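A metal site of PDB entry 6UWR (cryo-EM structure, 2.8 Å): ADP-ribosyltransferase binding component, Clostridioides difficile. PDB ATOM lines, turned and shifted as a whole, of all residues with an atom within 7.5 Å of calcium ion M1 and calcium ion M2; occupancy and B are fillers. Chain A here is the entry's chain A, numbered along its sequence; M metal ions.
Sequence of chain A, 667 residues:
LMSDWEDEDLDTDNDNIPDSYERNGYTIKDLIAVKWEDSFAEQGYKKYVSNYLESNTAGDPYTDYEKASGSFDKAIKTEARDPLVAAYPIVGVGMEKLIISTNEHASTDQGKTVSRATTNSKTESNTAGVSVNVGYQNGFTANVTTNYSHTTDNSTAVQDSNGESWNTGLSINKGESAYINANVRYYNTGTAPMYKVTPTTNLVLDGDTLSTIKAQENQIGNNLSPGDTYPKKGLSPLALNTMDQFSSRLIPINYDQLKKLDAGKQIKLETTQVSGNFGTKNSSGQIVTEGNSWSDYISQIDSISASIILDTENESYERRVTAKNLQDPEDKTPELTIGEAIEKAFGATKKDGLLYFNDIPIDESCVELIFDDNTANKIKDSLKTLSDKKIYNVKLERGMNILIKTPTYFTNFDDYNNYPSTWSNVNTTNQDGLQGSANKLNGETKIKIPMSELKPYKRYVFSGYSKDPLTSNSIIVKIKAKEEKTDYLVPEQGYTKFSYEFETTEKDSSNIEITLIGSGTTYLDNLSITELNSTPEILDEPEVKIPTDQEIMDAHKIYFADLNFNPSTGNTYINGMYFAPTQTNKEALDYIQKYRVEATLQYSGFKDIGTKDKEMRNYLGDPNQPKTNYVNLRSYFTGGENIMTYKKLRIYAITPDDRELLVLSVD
Six residues have an atom within 4 Å of calcium ion M1: Asp 13, Asp 15, Glu 22, Asn 51, Glu 54 and Asp 64.
The nearest printed residue that does not touch calcium ion M1 is Thr 57 (4.1 Å).
OD1 of Asp 64 lies within hydrogen-bond range of OG1 of Thr 57 (2.8 Å).
O of Asp 11 lies close to OD1 of Asn 14, at 3.3 Å.
The backbone NH of Ser 50 sits at hydrogen-bond distance from the backbone carbonyl oxygen of Glu 22 (3.2 Å).
The backbone NH of Asp 64 sits at hydrogen-bond distance from the backbone carbonyl oxygen of Ser 55 (2.9 Å).
The side-chain amide oxygen (OD1) of Asn 51 is in hydrogen-bond range of the backbone NH (N) of Leu 53 (3.0 Å).
N of Asn 51 sits at hydrogen-bond distance from OG1 of Thr 57.
The nearest printed residue that does not touch calcium ion M2 is Asp 19 (4.1 Å).
OD1 of Asp 13 binds calcium ion M2 (2.2 Å).
Calcium ion M2 is bound by O of Ile 17, 2.3 Å away.
OD1 of Asp 15 is bound to calcium ion M2, at 2.3 Å.
Calcium ion M2 is bound by OD1 of Asp 11 (2.4 Å).
Calcium ion M2 is bound by the side-chain carboxylate (OE2) of Glu 22 (2.5 Å).
Calcium ion M2 has five donor atoms within binding distance.
Calcium ion M1 is bound by OD2 of Asp 13 (2.2 Å), OD2 of Asp 64 (2.3 Å), O of Glu 54 (2.3 Å), O of Asn 51 (2.4 Å), OD2 of Asp 15 (2.7 Å), OE1 of Glu 22 (2.7 Å) and OE2 of Glu 22 (2.8 Å).
Calcium ion M1 has seven donor atoms within binding distance.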
ATOM      1  N   LEU A  10      -2.561  -6.061  30.091  1.00  0.00           N
ATOM      2  CA  LEU A  10      -4.001  -6.266  30.174  1.00  0.00           C
ATOM      3  C   LEU A  10      -4.686  -5.635  28.968  1.00  0.00           C
ATOM      4  O   LEU A  10      -4.197  -4.668  28.385  1.00  0.00           O
ATOM      5  CB  LEU A  10      -4.550  -5.664  31.461  1.00  0.00           C
ATOM      6  CG  LEU A  10      -5.191  -6.635  32.438  1.00  0.00           C
ATOM      7  CD1 LEU A  10      -5.777  -5.880  33.614  1.00  0.00           C
ATOM      8  CD2 LEU A  10      -6.266  -7.454  31.735  1.00  0.00           C
ATOM      9  N   ASP A  11      -5.832  -6.208  28.588  1.00  0.00           N
ATOM     10  CA  ASP A  11      -6.602  -5.712  27.450  1.00  0.00           C
ATOM     11  C   ASP A  11      -8.051  -6.128  27.675  1.00  0.00           C
ATOM     12  O   ASP A  11      -8.416  -7.276  27.400  1.00  0.00           O
ATOM     13  CB  ASP A  11      -6.054  -6.271  26.154  1.00  0.00           C
ATOM     14  CG  ASP A  11      -6.007  -5.252  25.067  1.00  0.00           C
ATOM     15  OD1 ASP A  11      -6.838  -4.321  25.073  1.00  0.00           O
ATOM     16  OD2 ASP A  11      -5.125  -5.375  24.197  1.00  0.00           O
ATOM     17  N   THR A  12      -8.867  -5.202  28.162  1.00  0.00           N
ATOM     18  CA  THR A  12     -10.229  -5.566  28.531  1.00  0.00           C
ATOM     19  C   THR A  12     -11.214  -5.306  27.394  1.00  0.00           C
ATOM     20  O   THR A  12     -12.193  -6.031  27.260  1.00  0.00           O
ATOM     21  CB  THR A  12     -10.649  -4.805  29.782  1.00  0.00           C
ATOM     22  OG1 THR A  12      -9.693  -3.797  30.068  1.00  0.00           O
ATOM     23  CG2 THR A  12     -10.706  -5.743  30.952  1.00  0.00           C
ATOM     24  N   ASP A  13     -10.979  -4.274  26.595  1.00  0.00           N
ATOM     25  CA  ASP A  13     -11.809  -4.000  25.439  1.00  0.00           C
ATOM     26  C   ASP A  13     -11.369  -4.757  24.208  1.00  0.00           C
ATOM     27  O   ASP A  13     -12.089  -4.772  23.214  1.00  0.00           O
ATOM     28  CB  ASP A  13     -11.823  -2.496  25.144  1.00  0.00           C
ATOM     29  CG  ASP A  13     -10.451  -1.928  24.951  1.00  0.00           C
ATOM     30  OD1 ASP A  13      -9.476  -2.567  25.366  1.00  0.00           O
ATOM     31  OD2 ASP A  13     -10.338  -0.830  24.376  1.00  0.00           O
ATOM     32  N   ASN A  14     -10.190  -5.381  24.254  1.00  0.00           N
ATOM     33  CA  ASN A  14      -9.728  -6.325  23.252  1.00  0.00           C
ATOM     34  C   ASN A  14      -9.406  -5.675  21.919  1.00  0.00           C
ATOM     35  O   ASN A  14      -9.398  -6.346  20.886  1.00  0.00           O
ATOM     36  CB  ASN A  14     -10.725  -7.466  23.060  1.00  0.00           C
ATOM     37  CG  ASN A  14     -10.598  -8.534  24.112  1.00  0.00           C
ATOM     38  OD1 ASN A  14      -9.505  -8.787  24.621  1.00  0.00           O
ATOM     39  ND2 ASN A  14     -11.704  -9.153  24.465  1.00  0.00           N
ATOM     40  N   ASP A  15      -9.134  -4.378  21.893  1.00  0.00           N
ATOM     41  CA  ASP A  15      -8.334  -3.858  20.798  1.00  0.00           C
ATOM     42  C   ASP A  15      -6.879  -4.187  21.126  1.00  0.00           C
ATOM     43  O   ASP A  15      -6.575  -4.819  22.140  1.00  0.00           O
ATOM     44  CB  ASP A  15      -8.580  -2.373  20.572  1.00  0.00           C
ATOM     45  CG  ASP A  15      -8.679  -1.600  21.849  1.00  0.00           C
ATOM     46  OD1 ASP A  15      -8.194  -2.060  22.890  1.00  0.00           O
ATOM     47  OD2 ASP A  15      -9.254  -0.493  21.816  1.00  0.00           O
ATOM     48  N   ASN A  16      -5.951  -3.791  20.259  1.00  0.00           N
ATOM     49  CA  ASN A  16      -4.572  -4.205  20.450  1.00  0.00           C
ATOM     50  C   ASN A  16      -3.756  -3.201  21.252  1.00  0.00           C
ATOM     51  O   ASN A  16      -2.537  -3.150  21.094  1.00  0.00           O
ATOM     52  CB  ASN A  16      -3.921  -4.452  19.085  1.00  0.00           C
ATOM     53  CG  ASN A  16      -4.693  -5.456  18.269  1.00  0.00           C
ATOM     54  OD1 ASN A  16      -5.432  -6.271  18.804  1.00  0.00           O
ATOM     55  ND2 ASN A  16      -4.521  -5.388  16.952  1.00  0.00           N
ATOM     56  N   ILE A  17      -4.401  -2.421  22.102  1.00  0.00           N
ATOM     57  CA  ILE A  17      -3.718  -1.454  22.967  1.00  0.00           C
ATOM     58  C   ILE A  17      -3.970  -1.877  24.411  1.00  0.00           C
ATOM     59  O   ILE A  17      -5.117  -2.098  24.793  1.00  0.00           O
ATOM     60  CB  ILE A  17      -4.224  -0.026  22.725  1.00  0.00           C
ATOM     61  CG1 ILE A  17      -4.380   0.239  21.236  1.00  0.00           C
ATOM     62  CG2 ILE A  17      -3.292   0.978  23.346  1.00  0.00           C
ATOM     63  CD1 ILE A  17      -5.176   1.465  20.928  1.00  0.00           C
ATOM     64  N   PRO A  18      -2.930  -1.996  25.231  1.00  0.00           N
ATOM     65  CA  PRO A  18      -3.144  -2.342  26.638  1.00  0.00           C
ATOM     66  C   PRO A  18      -3.821  -1.212  27.394  1.00  0.00           C
ATOM     67  O   PRO A  18      -3.864  -0.065  26.968  1.00  0.00           O
ATOM     68  CB  PRO A  18      -1.721  -2.589  27.154  1.00  0.00           C
ATOM     69  CG  PRO A  18      -0.924  -2.881  25.948  1.00  0.00           C
ATOM     70  CD  PRO A  18      -1.507  -2.045  24.866  1.00  0.00           C
ATOM     71  N   ASP A  19      -4.356  -1.563  28.567  1.00  0.00           N
ATOM     72  CA  ASP A  19      -5.124  -0.593  29.353  1.00  0.00           C
ATOM     73  C   ASP A  19      -4.266   0.569  29.817  1.00  0.00           C
ATOM     74  O   ASP A  19      -4.674   1.727  29.713  1.00  0.00           O
ATOM     75  CB  ASP A  19      -5.757  -1.287  30.554  1.00  0.00           C
ATOM     76  CG  ASP A  19      -6.664  -2.412  30.174  1.00  0.00           C
ATOM     77  OD1 ASP A  19      -6.681  -2.771  28.980  1.00  0.00           O
ATOM     78  OD2 ASP A  19      -7.346  -2.955  31.059  1.00  0.00           O
ATOM     79  N   SER A  20      -3.079   0.271  30.353  1.00  0.00           N
ATOM     80  CA  SER A  20      -2.187   1.317  30.819  1.00  0.00           C
ATOM     81  C   SER A  20      -1.795   2.287  29.718  1.00  0.00           C
ATOM     82  O   SER A  20      -1.681   3.480  29.984  1.00  0.00           O
ATOM     83  CB  SER A  20      -0.948   0.687  31.443  1.00  0.00           C
ATOM     84  OG  SER A  20      -0.589  -0.486  30.756  1.00  0.00           O
ATOM     85  N   GLU A  22      -3.668   3.054  27.099  1.00  0.00           N
ATOM     86  CA  GLU A  22      -4.829   3.866  26.794  1.00  0.00           C
ATOM     87  C   GLU A  22      -5.061   4.928  27.861  1.00  0.00           C
ATOM     88  O   GLU A  22      -5.526   6.021  27.543  1.00  0.00           O
ATOM     89  CB  GLU A  22      -6.063   2.985  26.662  1.00  0.00           C
ATOM     90  CG  GLU A  22      -5.943   1.951  25.591  1.00  0.00           C
ATOM     91  CD  GLU A  22      -7.242   1.710  24.877  1.00  0.00           C
ATOM     92  OE1 GLU A  22      -7.872   2.688  24.458  1.00  0.00           O
ATOM     93  OE2 GLU A  22      -7.633   0.541  24.727  1.00  0.00           O
ATOM     94  N   TYR A  26      -0.145   6.708  24.430  1.00  0.00           N
ATOM     95  CA  TYR A  26       0.576   5.784  23.578  1.00  0.00           C
ATOM     96  C   TYR A  26       0.733   6.401  22.196  1.00  0.00           C
ATOM     97  O   TYR A  26       0.217   7.486  21.912  1.00  0.00           O
ATOM     98  CB  TYR A  26      -0.139   4.434  23.486  1.00  0.00           C
ATOM     99  CG  TYR A  26      -1.505   4.521  22.836  1.00  0.00           C
ATOM    100  CD1 TYR A  26      -2.610   4.884  23.570  1.00  0.00           C
ATOM    101  CD2 TYR A  26      -1.671   4.236  21.499  1.00  0.00           C
ATOM    102  CE1 TYR A  26      -3.848   4.963  22.984  1.00  0.00           C
ATOM    103  CE2 TYR A  26      -2.898   4.323  20.911  1.00  0.00           C
ATOM    104  CZ  TYR A  26      -3.980   4.684  21.652  1.00  0.00           C
ATOM    105  OH  TYR A  26      -5.218   4.762  21.067  1.00  0.00           O
ATOM    106  N   SER A  50      -7.306   7.029  25.058  1.00  0.00           N
ATOM    107  CA  SER A  50      -8.609   6.513  24.662  1.00  0.00           C
ATOM    108  C   SER A  50      -9.215   5.759  25.839  1.00  0.00           C
ATOM    109  O   SER A  50      -8.655   5.726  26.938  1.00  0.00           O
ATOM    110  CB  SER A  50      -8.486   5.617  23.432  1.00  0.00           C
ATOM    111  OG  SER A  50      -7.308   4.841  23.483  1.00  0.00           O
ATOM    112  N   ASN A  51     -10.380   5.174  25.605  1.00  0.00           N
ATOM    113  CA  ASN A  51     -11.129   4.458  26.612  1.00  0.00           C
ATOM    114  C   ASN A  51     -10.658   3.007  26.640  1.00  0.00           C
ATOM    115  O   ASN A  51     -10.738   2.313  25.632  1.00  0.00           O
ATOM    116  CB  ASN A  51     -12.620   4.545  26.327  1.00  0.00           C
ATOM    117  CG  ASN A  51     -13.480   4.086  27.470  1.00  0.00           C
ATOM    118  OD1 ASN A  51     -13.008   3.402  28.373  1.00  0.00           O
ATOM    119  ND2 ASN A  51     -14.740   4.444  27.438  1.00  0.00           N
ATOM    120  N   TYR A  52     -10.150   2.563  27.787  1.00  0.00           N
ATOM    121  CA  TYR A  52      -9.639   1.210  27.894  1.00  0.00           C
ATOM    122  C   TYR A  52     -10.725   0.196  28.186  1.00  0.00           C
ATOM    123  O   TYR A  52     -10.425  -0.998  28.267  1.00  0.00           O
ATOM    124  CB  TYR A  52      -8.543   1.140  28.953  1.00  0.00           C
ATOM    125  CG  TYR A  52      -9.046   1.230  30.367  1.00  0.00           C
ATOM    126  CD1 TYR A  52      -9.298   2.447  30.954  1.00  0.00           C
ATOM    127  CD2 TYR A  52      -9.265   0.091  31.125  1.00  0.00           C
ATOM    128  CE1 TYR A  52      -9.752   2.534  32.247  1.00  0.00           C
ATOM    129  CE2 TYR A  52      -9.721   0.163  32.402  1.00  0.00           C
ATOM    130  CZ  TYR A  52      -9.963   1.380  32.957  1.00  0.00           C
ATOM    131  OH  TYR A  52     -10.417   1.467  34.250  1.00  0.00           O
ATOM    132  N   LEU A  53     -11.956   0.641  28.372  1.00  0.00           N
ATOM    133  CA  LEU A  53     -13.104  -0.248  28.513  1.00  0.00           C
ATOM    134  C   LEU A  53     -14.012  -0.200  27.296  1.00  0.00           C
ATOM    135  O   LEU A  53     -15.084  -0.799  27.299  1.00  0.00           O
ATOM    136  CB  LEU A  53     -13.905   0.117  29.767  1.00  0.00           C
ATOM    137  CG  LEU A  53     -13.326  -0.267  31.126  1.00  0.00           C
ATOM    138  CD1 LEU A  53     -14.248   0.218  32.199  1.00  0.00           C
ATOM    139  CD2 LEU A  53     -13.152  -1.765  31.214  1.00  0.00           C
ATOM    140  N   GLU A  54     -13.600   0.509  26.247  1.00  0.00           N
ATOM    141  CA  GLU A  54     -14.382   0.689  25.043  1.00  0.00           C
ATOM    142  C   GLU A  54     -13.481   0.403  23.852  1.00  0.00           C
ATOM    143  O   GLU A  54     -12.387   0.952  23.766  1.00  0.00           O
ATOM    144  CB  GLU A  54     -14.923   2.117  24.960  1.00  0.00           C
ATOM    145  CG  GLU A  54     -16.202   2.251  24.177  1.00  0.00           C
ATOM    146  CD  GLU A  54     -17.378   1.590  24.859  1.00  0.00           C
ATOM    147  OE1 GLU A  54     -17.800   2.069  25.932  1.00  0.00           O
ATOM    148  OE2 GLU A  54     -17.886   0.583  24.317  1.00  0.00           O
ATOM    149  N   SER A  55     -13.944  -0.445  22.947  1.00  0.00           N
ATOM    150  CA  SER A  55     -13.154  -0.744  21.760  1.00  0.00           C
ATOM    151  C   SER A  55     -13.246   0.367  20.734  1.00  0.00           C
ATOM    152  O   SER A  55     -12.306   0.568  19.962  1.00  0.00           O
ATOM    153  CB  SER A  55     -13.591  -2.071  21.160  1.00  0.00           C
ATOM    154  OG  SER A  55     -12.646  -2.539  20.235  1.00  0.00           O
ATOM    155  N   ASN A  56     -14.365   1.083  20.717  1.00  0.00           N
ATOM    156  CA  ASN A  56     -14.594   2.218  19.826  1.00  0.00           C
ATOM    157  C   ASN A  56     -14.892   3.404  20.725  1.00  0.00           C
ATOM    158  O   ASN A  56     -16.031   3.610  21.130  1.00  0.00           O
ATOM    159  CB  ASN A  56     -15.751   1.956  18.858  1.00  0.00           C
ATOM    160  CG  ASN A  56     -15.451   0.859  17.864  1.00  0.00           C
ATOM    161  OD1 ASN A  56     -15.375   1.109  16.674  1.00  0.00           O
ATOM    162  ND2 ASN A  56     -15.301  -0.359  18.352  1.00  0.00           N
ATOM    163  N   THR A  57     -13.862   4.183  21.051  1.00  0.00           N
ATOM    164  CA  THR A  57     -14.035   5.273  21.998  1.00  0.00           C
ATOM    165  C   THR A  57     -14.948   6.350  21.436  1.00  0.00           C
ATOM    166  O   THR A  57     -15.871   6.818  22.121  1.00  0.00           O
ATOM    167  CB  THR A  57     -12.677   5.870  22.359  1.00  0.00           C
ATOM    168  OG1 THR A  57     -11.844   4.849  22.908  1.00  0.00           O
ATOM    169  CG2 THR A  57     -12.839   6.979  23.374  1.00  0.00           C
ATOM    170  N   THR A  63     -12.280   0.936  15.324  1.00  0.00           N
ATOM    171  CA  THR A  63     -11.787   0.758  16.672  1.00  0.00           C
ATOM    172  C   THR A  63     -10.654   1.728  16.969  1.00  0.00           C
ATOM    173  O   THR A  63     -10.116   2.380  16.072  1.00  0.00           O
ATOM    174  CB  THR A  63     -11.312  -0.684  16.898  1.00  0.00           C
ATOM    175  OG1 THR A  63     -10.080  -0.891  16.222  1.00  0.00           O
ATOM    176  CG2 THR A  63     -12.323  -1.655  16.371  1.00  0.00           C
ATOM    177  N   ASP A  64     -10.293   1.824  18.243  1.00  0.00           N
ATOM    178  CA  ASP A  64      -9.217   2.737  18.644  1.00  0.00           C
ATOM    179  C   ASP A  64      -7.914   2.405  17.935  1.00  0.00           C
ATOM    180  O   ASP A  64      -7.182   3.326  17.545  1.00  0.00           O
ATOM    181  CB  ASP A  64      -9.021   2.676  20.156  1.00  0.00           C
ATOM    182  CG  ASP A  64     -10.146   3.310  20.907  1.00  0.00           C
ATOM    183  OD1 ASP A  64     -10.812   4.189  20.344  1.00  0.00           O
ATOM    184  OD2 ASP A  64     -10.368   2.945  22.069  1.00  0.00           O
ATOM    185  N   TYR A  65      -7.619   1.127  17.752  1.00  0.00           N
ATOM    186  CA  TYR A  65      -6.389   0.747  17.078  1.00  0.00           C
ATOM    187  C   TYR A  65      -6.421   1.100  15.594  1.00  0.00           C
ATOM    188  O   TYR A  65      -5.447   1.621  15.061  1.00  0.00           O
ATOM    189  CB  TYR A  65      -6.102  -0.732  17.260  1.00  0.00           C
ATOM    190  CG  TYR A  65      -4.833  -1.149  16.576  1.00  0.00           C
ATOM    191  CD1 TYR A  65      -3.606  -0.898  17.155  1.00  0.00           C
ATOM    192  CD2 TYR A  65      -4.860  -1.764  15.340  1.00  0.00           C
ATOM    193  CE1 TYR A  65      -2.448  -1.254  16.540  1.00  0.00           C
ATOM    194  CE2 TYR A  65      -3.699  -2.126  14.713  1.00  0.00           C
ATOM    195  CZ  TYR A  65      -2.489  -1.870  15.318  1.00  0.00           C
ATOM    196  OH  TYR A  65      -1.328  -2.233  14.692  1.00  0.00           O
ATOM    197  N   PRO A  83      -8.280   8.607  18.679  1.00  0.00           N
ATOM    198  CA  PRO A  83      -9.508   7.925  19.090  1.00  0.00           C
ATOM    199  C   PRO A  83     -10.570   8.831  19.702  1.00  0.00           C
ATOM    200  O   PRO A  83     -11.641   8.334  20.050  1.00  0.00           O
ATOM    201  CB  PRO A  83      -9.007   6.912  20.114  1.00  0.00           C
ATOM    202  CG  PRO A  83      -7.605   6.694  19.760  1.00  0.00           C
ATOM    203  CD  PRO A  83      -7.099   8.016  19.322  1.00  0.00           C
HETATM  204 CA    CA M   1     -10.064   1.264  23.632  1.00  0.00          CA
HETATM  205 CA    CA M   2      -7.375  -1.938  25.066  1.00  0.00          CA
